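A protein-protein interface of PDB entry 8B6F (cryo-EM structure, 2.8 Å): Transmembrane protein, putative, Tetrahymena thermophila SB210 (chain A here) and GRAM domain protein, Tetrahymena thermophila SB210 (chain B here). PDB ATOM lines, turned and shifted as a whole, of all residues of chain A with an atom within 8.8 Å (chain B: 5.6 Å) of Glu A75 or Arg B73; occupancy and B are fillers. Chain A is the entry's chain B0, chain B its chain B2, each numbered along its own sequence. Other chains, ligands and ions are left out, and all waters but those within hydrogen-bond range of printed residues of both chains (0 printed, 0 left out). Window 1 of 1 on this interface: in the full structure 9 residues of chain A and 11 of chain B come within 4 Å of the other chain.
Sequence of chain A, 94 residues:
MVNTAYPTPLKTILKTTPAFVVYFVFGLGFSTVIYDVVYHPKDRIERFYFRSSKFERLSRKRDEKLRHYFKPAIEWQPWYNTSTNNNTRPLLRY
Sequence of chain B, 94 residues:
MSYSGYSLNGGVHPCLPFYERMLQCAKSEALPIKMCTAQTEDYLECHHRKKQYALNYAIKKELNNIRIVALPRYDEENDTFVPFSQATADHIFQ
The guanidinium group (NH1) of Arg B73 lies within salt-bridge range of the side-chain carboxylate (OE1) of Glu A75 (3.7 Å).
The side-chain amide oxygen of Gln A77 lies within hydrogen-bond range of the backbone NH of Leu B71 (2.8 Å).
The side-chain amide nitrogen (NE2) of Gln A77 sits close to the guanidinium group (NH1) of Arg B73, 3.0 Å away.
OH of Tyr A80 sits at hydrogen-bond distance from NH2 of Arg B73 (2.8 Å).
Of chain B, only Arg B73 and Tyr B74 come within 4 Å of Glu A75.
Of chain A, only Glu A75, Gln A77 and Tyr A80 come within 4 Å of Arg B73.
No residue of chain A comes within 4 Å of Pro B72.
Of the printed residues of chain A, Ile B92 touches Tyr A80 (3.6 Å).
Printed residues of chain B within 4 Å of Pro A78: Leu B71 (3.7 Å).
Of the printed residues of chain A, Tyr B74 touches Ile A74 and Glu A75.
Of the printed residues of chain B, Ile A74 touches Tyr B74 (3.3 Å).
Printed residues of chain A within 4 Å of Leu B71: Gln A77 (2.8 Å) and Pro A78 (3.7 Å).
The nearest residue of chain A that does not touch Arg B73 is Trp A76 (4.3 Å).
Tyr B74 touches Ile A74 (CB to CG1, 3.3 Å).
Glu A75 touches Tyr B74 (OE1 to N, 3.8 Å).
NE2 of Gln A77 touches CD2 of Phe B84 (3.1 Å).
CD1 of Leu B71 touches CD of Pro A78 (3.7 Å).
Tyr A80 touches Ile B92.
Printed residues of chain A that touch a printed residue of chain B: Ile A74, Glu A75, Gln A77, Pro A78 and Tyr A80.
Hydrophobic or aromatic side chains of chain A within 4 Å of the printed part of chain B: Ile A74, Pro A78 and Tyr A80.
Among the printed residues, Asp or Glu carboxylates within 4 Å of a Lys or Arg side-chain nitrogen of the other chain: Glu A75 with Arg B73.
O of Arg B73 lies within hydrogen-bond range of N of Val B82 (2.8 Å).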
ATOM      1  N   TYR A  69     -29.851  25.763   8.513  1.00  0.00           N
ATOM      2  CA  TYR A  69     -29.955  24.327   8.282  1.00  0.00           C
ATOM      3  C   TYR A  69     -30.036  23.967   6.809  1.00  0.00           C
ATOM      4  O   TYR A  69     -29.306  23.079   6.355  1.00  0.00           O
ATOM      5  CB  TYR A  69     -31.177  23.763   9.026  1.00  0.00           C
ATOM      6  CG  TYR A  69     -30.981  23.684  10.521  1.00  0.00           C
ATOM      7  CD1 TYR A  69     -30.437  22.550  11.107  1.00  0.00           C
ATOM      8  CD2 TYR A  69     -31.329  24.745  11.345  1.00  0.00           C
ATOM      9  CE1 TYR A  69     -30.249  22.471  12.470  1.00  0.00           C
ATOM     10  CE2 TYR A  69     -31.144  24.676  12.711  1.00  0.00           C
ATOM     11  CZ  TYR A  69     -30.604  23.536  13.266  1.00  0.00           C
ATOM     12  OH  TYR A  69     -30.417  23.459  14.626  1.00  0.00           O
ATOM     13  N   PHE A  70     -30.907  24.627   6.046  1.00  0.00           N
ATOM     14  CA  PHE A  70     -31.112  24.234   4.656  1.00  0.00           C
ATOM     15  C   PHE A  70     -29.829  24.362   3.845  1.00  0.00           C
ATOM     16  O   PHE A  70     -29.439  23.435   3.127  1.00  0.00           O
ATOM     17  CB  PHE A  70     -32.224  25.078   4.035  1.00  0.00           C
ATOM     18  CG  PHE A  70     -32.259  25.024   2.538  1.00  0.00           C
ATOM     19  CD1 PHE A  70     -32.868  23.971   1.882  1.00  0.00           C
ATOM     20  CD2 PHE A  70     -31.690  26.038   1.787  1.00  0.00           C
ATOM     21  CE1 PHE A  70     -32.902  23.927   0.501  1.00  0.00           C
ATOM     22  CE2 PHE A  70     -31.723  25.999   0.408  1.00  0.00           C
ATOM     23  CZ  PHE A  70     -32.329  24.942  -0.235  1.00  0.00           C
ATOM     24  N   LYS A  71     -29.150  25.504   3.951  1.00  0.00           N
ATOM     25  CA  LYS A  71     -27.957  25.720   3.136  1.00  0.00           C
ATOM     26  C   LYS A  71     -26.839  24.749   3.478  1.00  0.00           C
ATOM     27  O   LYS A  71     -26.276  24.139   2.553  1.00  0.00           O
ATOM     28  CB  LYS A  71     -27.498  27.174   3.271  1.00  0.00           C
ATOM     29  CG  LYS A  71     -28.184  28.125   2.301  1.00  0.00           C
ATOM     30  CD  LYS A  71     -27.761  27.866   0.861  1.00  0.00           C
ATOM     31  CE  LYS A  71     -28.376  28.884  -0.082  1.00  0.00           C
ATOM     32  NZ  LYS A  71     -27.993  28.633  -1.498  1.00  0.00           N
ATOM     33  N   PRO A  72     -26.461  24.554   4.742  1.00  0.00           N
ATOM     34  CA  PRO A  72     -25.478  23.498   5.034  1.00  0.00           C
ATOM     35  C   PRO A  72     -25.939  22.123   4.590  1.00  0.00           C
ATOM     36  O   PRO A  72     -25.125  21.318   4.124  1.00  0.00           O
ATOM     37  CB  PRO A  72     -25.314  23.589   6.558  1.00  0.00           C
ATOM     38  CG  PRO A  72     -25.674  24.988   6.892  1.00  0.00           C
ATOM     39  CD  PRO A  72     -26.757  25.374   5.929  1.00  0.00           C
ATOM     40  N   ALA A  73     -27.232  21.828   4.734  1.00  0.00           N
ATOM     41  CA  ALA A  73     -27.735  20.518   4.336  1.00  0.00           C
ATOM     42  C   ALA A  73     -27.570  20.294   2.839  1.00  0.00           C
ATOM     43  O   ALA A  73     -27.195  19.198   2.406  1.00  0.00           O
ATOM     44  CB  ALA A  73     -29.203  20.379   4.738  1.00  0.00           C
ATOM     45  N   ILE A  74     -27.844  21.319   2.033  1.00  0.00           N
ATOM     46  CA  ILE A  74     -27.804  21.169   0.582  1.00  0.00           C
ATOM     47  C   ILE A  74     -26.405  21.357   0.006  1.00  0.00           C
ATOM     48  O   ILE A  74     -26.149  20.917  -1.123  1.00  0.00           O
ATOM     49  CB  ILE A  74     -28.794  22.147  -0.082  1.00  0.00           C
ATOM     50  CG1 ILE A  74     -29.095  21.726  -1.523  1.00  0.00           C
ATOM     51  CG2 ILE A  74     -28.257  23.571  -0.064  1.00  0.00           C
ATOM     52  CD1 ILE A  74     -29.827  20.410  -1.656  1.00  0.00           C
ATOM     53  N   GLU A  75     -25.499  21.999   0.739  1.00  0.00           N
ATOM     54  CA  GLU A  75     -24.105  22.116   0.340  1.00  0.00           C
ATOM     55  C   GLU A  75     -23.211  21.125   1.069  1.00  0.00           C
ATOM     56  O   GLU A  75     -21.984  21.233   0.990  1.00  0.00           O
ATOM     57  CB  GLU A  75     -23.605  23.541   0.586  1.00  0.00           C
ATOM     58  CG  GLU A  75     -24.451  24.630  -0.060  1.00  0.00           C
ATOM     59  CD  GLU A  75     -24.478  24.543  -1.575  1.00  0.00           C
ATOM     60  OE1 GLU A  75     -24.864  23.483  -2.110  1.00  0.00           O
ATOM     61  OE2 GLU A  75     -24.111  25.539  -2.233  1.00  0.00           O
ATOM     62  N   TRP A  76     -23.798  20.165   1.780  1.00  0.00           N
ATOM     63  CA  TRP A  76     -23.018  19.211   2.552  1.00  0.00           C
ATOM     64  C   TRP A  76     -22.087  18.408   1.655  1.00  0.00           C
ATOM     65  O   TRP A  76     -22.450  18.014   0.544  1.00  0.00           O
ATOM     66  CB  TRP A  76     -23.949  18.268   3.309  1.00  0.00           C
ATOM     67  CG  TRP A  76     -23.233  17.205   4.078  1.00  0.00           C
ATOM     68  CD1 TRP A  76     -22.597  17.346   5.274  1.00  0.00           C
ATOM     69  CD2 TRP A  76     -23.085  15.830   3.704  1.00  0.00           C
ATOM     70  NE1 TRP A  76     -22.060  16.146   5.669  1.00  0.00           N
ATOM     71  CE2 TRP A  76     -22.346  15.199   4.722  1.00  0.00           C
ATOM     72  CE3 TRP A  76     -23.505  15.073   2.607  1.00  0.00           C
ATOM     73  CZ2 TRP A  76     -22.017  13.846   4.676  1.00  0.00           C
ATOM     74  CZ3 TRP A  76     -23.178  13.730   2.562  1.00  0.00           C
ATOM     75  CH2 TRP A  76     -22.440  13.131   3.590  1.00  0.00           C
ATOM     76  N   GLN A  77     -20.880  18.165   2.153  1.00  0.00           N
ATOM     77  CA  GLN A  77     -19.922  17.260   1.544  1.00  0.00           C
ATOM     78  C   GLN A  77     -19.415  16.296   2.603  1.00  0.00           C
ATOM     79  O   GLN A  77     -19.396  16.631   3.791  1.00  0.00           O
ATOM     80  CB  GLN A  77     -18.736  18.020   0.932  1.00  0.00           C
ATOM     81  CG  GLN A  77     -19.120  18.999  -0.162  1.00  0.00           C
ATOM     82  CD  GLN A  77     -19.612  18.309  -1.414  1.00  0.00           C
ATOM     83  OE1 GLN A  77     -19.707  17.086  -1.467  1.00  0.00           O
ATOM     84  NE2 GLN A  77     -19.927  19.095  -2.436  1.00  0.00           N
ATOM     85  N   PRO A  78     -18.988  15.096   2.206  1.00  0.00           N
ATOM     86  CA  PRO A  78     -18.539  14.120   3.213  1.00  0.00           C
ATOM     87  C   PRO A  78     -17.386  14.624   4.056  1.00  0.00           C
ATOM     88  O   PRO A  78     -17.238  14.198   5.208  1.00  0.00           O
ATOM     89  CB  PRO A  78     -18.136  12.901   2.371  1.00  0.00           C
ATOM     90  CG  PRO A  78     -18.847  13.071   1.078  1.00  0.00           C
ATOM     91  CD  PRO A  78     -18.920  14.544   0.843  1.00  0.00           C
ATOM     92  N   TRP A  79     -16.569  15.527   3.522  1.00  0.00           N
ATOM     93  CA  TRP A  79     -15.380  16.012   4.206  1.00  0.00           C
ATOM     94  C   TRP A  79     -15.581  17.387   4.834  1.00  0.00           C
ATOM     95  O   TRP A  79     -14.617  17.973   5.336  1.00  0.00           O
ATOM     96  CB  TRP A  79     -14.188  16.030   3.241  1.00  0.00           C
ATOM     97  CG  TRP A  79     -14.516  16.475   1.845  1.00  0.00           C
ATOM     98  CD1 TRP A  79     -15.068  15.717   0.853  1.00  0.00           C
ATOM     99  CD2 TRP A  79     -14.305  17.776   1.283  1.00  0.00           C
ATOM    100  NE1 TRP A  79     -15.215  16.465  -0.289  1.00  0.00           N
ATOM    101  CE2 TRP A  79     -14.755  17.733  -0.051  1.00  0.00           C
ATOM    102  CE3 TRP A  79     -13.781  18.972   1.780  1.00  0.00           C
ATOM    103  CZ2 TRP A  79     -14.697  18.839  -0.894  1.00  0.00           C
ATOM    104  CZ3 TRP A  79     -13.724  20.069   0.943  1.00  0.00           C
ATOM    105  CH2 TRP A  79     -14.179  19.995  -0.381  1.00  0.00           C
ATOM    106  N   TYR A  80     -16.807  17.919   4.811  1.00  0.00           N
ATOM    107  CA  TYR A  80     -17.091  19.163   5.520  1.00  0.00           C
ATOM    108  C   TYR A  80     -17.235  18.956   7.020  1.00  0.00           C
ATOM    109  O   TYR A  80     -16.858  19.839   7.797  1.00  0.00           O
ATOM    110  CB  TYR A  80     -18.360  19.824   4.975  1.00  0.00           C
ATOM    111  CG  TYR A  80     -18.180  20.532   3.654  1.00  0.00           C
ATOM    112  CD1 TYR A  80     -16.944  20.570   3.026  1.00  0.00           C
ATOM    113  CD2 TYR A  80     -19.237  21.207   3.061  1.00  0.00           C
ATOM    114  CE1 TYR A  80     -16.770  21.228   1.839  1.00  0.00           C
ATOM    115  CE2 TYR A  80     -19.071  21.873   1.864  1.00  0.00           C
ATOM    116  CZ  TYR A  80     -17.825  21.887   1.268  1.00  0.00           C
ATOM    117  OH  TYR A  80     -17.612  22.534   0.080  1.00  0.00           O
ATOM    118  N   ASN A  81     -17.776  17.821   7.446  1.00  0.00           N
ATOM    119  CA  ASN A  81     -17.995  17.599   8.867  1.00  0.00           C
ATOM    120  C   ASN A  81     -16.672  17.561   9.615  1.00  0.00           C
ATOM    121  O   ASN A  81     -15.677  17.018   9.128  1.00  0.00           O
ATOM    122  CB  ASN A  81     -18.761  16.296   9.089  1.00  0.00           C
ATOM    123  CG  ASN A  81     -20.145  16.329   8.485  1.00  0.00           C
ATOM    124  OD1 ASN A  81     -20.358  15.859   7.368  1.00  0.00           O
ATOM    125  ND2 ASN A  81     -21.097  16.895   9.218  1.00  0.00           N
ATOM    126  N   LEU B  71     -20.297  15.622  -3.741  1.00  0.00           N
ATOM    127  CA  LEU B  71     -21.656  15.676  -4.255  1.00  0.00           C
ATOM    128  C   LEU B  71     -21.845  16.910  -5.135  1.00  0.00           C
ATOM    129  O   LEU B  71     -21.138  17.908  -4.977  1.00  0.00           O
ATOM    130  CB  LEU B  71     -22.662  15.711  -3.109  1.00  0.00           C
ATOM    131  CG  LEU B  71     -22.890  14.421  -2.318  1.00  0.00           C
ATOM    132  CD1 LEU B  71     -21.645  13.993  -1.569  1.00  0.00           C
ATOM    133  CD2 LEU B  71     -24.048  14.610  -1.357  1.00  0.00           C
ATOM    134  N   PRO B  72     -22.796  16.869  -6.067  1.00  0.00           N
ATOM    135  CA  PRO B  72     -23.048  18.046  -6.905  1.00  0.00           C
ATOM    136  C   PRO B  72     -23.618  19.201  -6.101  1.00  0.00           C
ATOM    137  O   PRO B  72     -24.394  19.009  -5.163  1.00  0.00           O
ATOM    138  CB  PRO B  72     -24.059  17.537  -7.938  1.00  0.00           C
ATOM    139  CG  PRO B  72     -24.747  16.415  -7.258  1.00  0.00           C
ATOM    140  CD  PRO B  72     -23.719  15.765  -6.380  1.00  0.00           C
ATOM    141  N   ARG B  73     -23.225  20.413  -6.481  1.00  0.00           N
ATOM    142  CA  ARG B  73     -23.802  21.602  -5.881  1.00  0.00           C
ATOM    143  C   ARG B  73     -25.228  21.812  -6.376  1.00  0.00           C
ATOM    144  O   ARG B  73     -25.615  21.363  -7.458  1.00  0.00           O
ATOM    145  CB  ARG B  73     -22.949  22.830  -6.199  1.00  0.00           C
ATOM    146  CG  ARG B  73     -21.748  22.961  -5.299  1.00  0.00           C
ATOM    147  CD  ARG B  73     -22.167  23.519  -3.955  1.00  0.00           C
ATOM    148  NE  ARG B  73     -21.140  23.309  -2.947  1.00  0.00           N
ATOM    149  CZ  ARG B  73     -21.070  22.248  -2.155  1.00  0.00           C
ATOM    150  NH1 ARG B  73     -21.953  21.267  -2.227  1.00  0.00           N
ATOM    151  NH2 ARG B  73     -20.084  22.166  -1.274  1.00  0.00           N
ATOM    152  N   TYR B  74     -26.013  22.514  -5.565  1.00  0.00           N
ATOM    153  CA  TYR B  74     -27.413  22.788  -5.864  1.00  0.00           C
ATOM    154  C   TYR B  74     -27.548  24.258  -6.236  1.00  0.00           C
ATOM    155  O   TYR B  74     -27.331  25.139  -5.398  1.00  0.00           O
ATOM    156  CB  TYR B  74     -28.307  22.441  -4.677  1.00  0.00           C
ATOM    157  CG  TYR B  74     -29.757  22.804  -4.894  1.00  0.00           C
ATOM    158  CD1 TYR B  74     -30.531  22.119  -5.822  1.00  0.00           C
ATOM    159  CD2 TYR B  74     -30.354  23.825  -4.168  1.00  0.00           C
ATOM    160  CE1 TYR B  74     -31.856  22.442  -6.026  1.00  0.00           C
ATOM    161  CE2 TYR B  74     -31.679  24.157  -4.364  1.00  0.00           C
ATOM    162  CZ  TYR B  74     -32.426  23.462  -5.294  1.00  0.00           C
ATOM    163  OH  TYR B  74     -33.747  23.787  -5.494  1.00  0.00           O
ATOM    164  N   ASP B  75     -27.905  24.515  -7.490  1.00  0.00           N
ATOM    165  CA  ASP B  75     -28.224  25.863  -7.945  1.00  0.00           C
ATOM    166  C   ASP B  75     -29.675  26.132  -7.575  1.00  0.00           C
ATOM    167  O   ASP B  75     -30.597  25.643  -8.229  1.00  0.00           O
ATOM    168  CB  ASP B  75     -27.988  25.998  -9.443  1.00  0.00           C
ATOM    169  CG  ASP B  75     -28.299  27.386  -9.957  1.00  0.00           C
ATOM    170  OD1 ASP B  75     -28.560  28.281  -9.127  1.00  0.00           O
ATOM    171  OD2 ASP B  75     -28.282  27.583 -11.189  1.00  0.00           O
ATOM    172  N   THR B  80     -31.735  23.440  -9.885  1.00  0.00           N
ATOM    173  CA  THR B  80     -31.015  22.409 -10.614  1.00  0.00           C
ATOM    174  C   THR B  80     -29.825  21.949  -9.786  1.00  0.00           C
ATOM    175  O   THR B  80     -29.516  22.510  -8.733  1.00  0.00           O
ATOM    176  CB  THR B  80     -30.540  22.913 -11.984  1.00  0.00           C
ATOM    177  OG1 THR B  80     -29.707  24.066 -11.812  1.00  0.00           O
ATOM    178  CG2 THR B  80     -31.726  23.274 -12.863  1.00  0.00           C
ATOM    179  N   PHE B  81     -29.155  20.911 -10.278  1.00  0.00           N
ATOM    180  CA  PHE B  81     -27.927  20.402  -9.682  1.00  0.00           C
ATOM    181  C   PHE B  81     -26.802  20.505 -10.699  1.00  0.00           C
ATOM    182  O   PHE B  81     -26.942  20.053 -11.839  1.00  0.00           O
ATOM    183  CB  PHE B  81     -28.094  18.956  -9.211  1.00  0.00           C
ATOM    184  CG  PHE B  81     -28.851  18.827  -7.921  1.00  0.00           C
ATOM    185  CD1 PHE B  81     -28.207  18.999  -6.709  1.00  0.00           C
ATOM    186  CD2 PHE B  81     -30.204  18.534  -7.920  1.00  0.00           C
ATOM    187  CE1 PHE B  81     -28.895  18.882  -5.519  1.00  0.00           C
ATOM    188  CE2 PHE B  81     -30.900  18.416  -6.733  1.00  0.00           C
ATOM    189  CZ  PHE B  81     -30.244  18.591  -5.531  1.00  0.00           C
ATOM    190  N   VAL B  82     -25.692  21.103 -10.280  1.00  0.00           N
ATOM    191  CA  VAL B  82     -24.529  21.309 -11.137  1.00  0.00           C
ATOM    192  C   VAL B  82     -23.381  20.493 -10.552  1.00  0.00           C
ATOM    193  O   VAL B  82     -23.252  20.412  -9.323  1.00  0.00           O
ATOM    194  CB  VAL B  82     -24.180  22.803 -11.236  1.00  0.00           C
ATOM    195  CG1 VAL B  82     -23.818  23.365  -9.868  1.00  0.00           C
ATOM    196  CG2 VAL B  82     -23.056  23.035 -12.227  1.00  0.00           C
ATOM    197  N   PRO B  83     -22.537  19.862 -11.371  1.00  0.00           N
ATOM    198  CA  PRO B  83     -21.437  19.073 -10.807  1.00  0.00           C
ATOM    199  C   PRO B  83     -20.497  19.932  -9.974  1.00  0.00           C
ATOM    200  O   PRO B  83     -20.284  21.113 -10.253  1.00  0.00           O
ATOM    201  CB  PRO B  83     -20.730  18.505 -12.045  1.00  0.00           C
ATOM    202  CG  PRO B  83     -21.186  19.354 -13.181  1.00  0.00           C
ATOM    203  CD  PRO B  83     -22.576  19.766 -12.839  1.00  0.00           C
ATOM    204  N   PHE B  84     -19.935  19.315  -8.932  1.00  0.00           N
ATOM    205  CA  PHE B  84     -19.005  20.023  -8.061  1.00  0.00           C
ATOM    206  C   PHE B  84     -17.810  20.556  -8.837  1.00  0.00           C
ATOM    207  O   PHE B  84     -17.219  21.569  -8.448  1.00  0.00           O
ATOM    208  CB  PHE B  84     -18.536  19.095  -6.940  1.00  0.00           C
ATOM    209  CG  PHE B  84     -17.647  19.762  -5.928  1.00  0.00           C
ATOM    210  CD1 PHE B  84     -16.282  19.866  -6.143  1.00  0.00           C
ATOM    211  CD2 PHE B  84     -18.176  20.271  -4.755  1.00  0.00           C
ATOM    212  CE1 PHE B  84     -15.463  20.474  -5.211  1.00  0.00           C
ATOM    213  CE2 PHE B  84     -17.363  20.880  -3.818  1.00  0.00           C
ATOM    214  CZ  PHE B  84     -16.006  20.982  -4.046  1.00  0.00           C
ATOM    215  N   THR B  88     -19.012  28.020  -9.745  1.00  0.00           N
ATOM    216  CA  THR B  88     -20.176  28.890  -9.656  1.00  0.00           C
ATOM    217  C   THR B  88     -19.878  30.032  -8.697  1.00  0.00           C
ATOM    218  O   THR B  88     -18.986  29.942  -7.850  1.00  0.00           O
ATOM    219  CB  THR B  88     -21.427  28.128  -9.194  1.00  0.00           C
ATOM    220  OG1 THR B  88     -21.183  27.524  -7.917  1.00  0.00           O
ATOM    221  CG2 THR B  88     -21.800  27.051 -10.201  1.00  0.00           C
ATOM    222  N   ASP B  90     -21.763  31.119  -6.283  1.00  0.00           N
ATOM    223  CA  ASP B  90     -22.139  30.729  -4.930  1.00  0.00           C
ATOM    224  C   ASP B  90     -21.247  29.635  -4.357  1.00  0.00           C
ATOM    225  O   ASP B  90     -21.407  29.284  -3.183  1.00  0.00           O
ATOM    226  CB  ASP B  90     -23.597  30.258  -4.912  1.00  0.00           C
ATOM    227  CG  ASP B  90     -24.540  31.255  -5.555  1.00  0.00           C
ATOM    228  OD1 ASP B  90     -24.244  32.468  -5.518  1.00  0.00           O
ATOM    229  OD2 ASP B  90     -25.579  30.828  -6.102  1.00  0.00           O
ATOM    230  N   HIS B  91     -20.322  29.093  -5.146  1.00  0.00           N
ATOM    231  CA  HIS B  91     -19.470  28.013  -4.667  1.00  0.00           C
ATOM    232  C   HIS B  91     -18.643  28.477  -3.475  1.00  0.00           C
ATOM    233  O   HIS B  91     -18.184  29.621  -3.421  1.00  0.00           O
ATOM    234  CB  HIS B  91     -18.552  27.532  -5.794  1.00  0.00           C
ATOM    235  CG  HIS B  91     -18.038  26.138  -5.601  1.00  0.00           C
ATOM    236  ND1 HIS B  91     -16.842  25.865  -4.973  1.00  0.00           N
ATOM    237  CD2 HIS B  91     -18.558  24.940  -5.957  1.00  0.00           C
ATOM    238  CE1 HIS B  91     -16.649  24.558  -4.950  1.00  0.00           C
ATOM    239  NE2 HIS B  91     -17.675  23.974  -5.541  1.00  0.00           N
ATOM    240  N   ILE B  92     -18.458  27.576  -2.507  1.00  0.00           N
ATOM    241  CA  ILE B  92     -17.713  27.921  -1.298  1.00  0.00           C
ATOM    242  C   ILE B  92     -16.263  28.236  -1.639  1.00  0.00           C
ATOM    243  O   ILE B  92     -15.691  29.219  -1.155  1.00  0.00           O
ATOM    244  CB  ILE B  92     -17.818  26.786  -0.262  1.00  0.00           C
ATOM    245  CG1 ILE B  92     -19.269  26.634   0.203  1.00  0.00           C
ATOM    246  CG2 ILE B  92     -16.893  27.051   0.926  1.00  0.00           C
ATOM    247  CD1 ILE B  92     -19.510  25.448   1.119  1.00  0.00           C
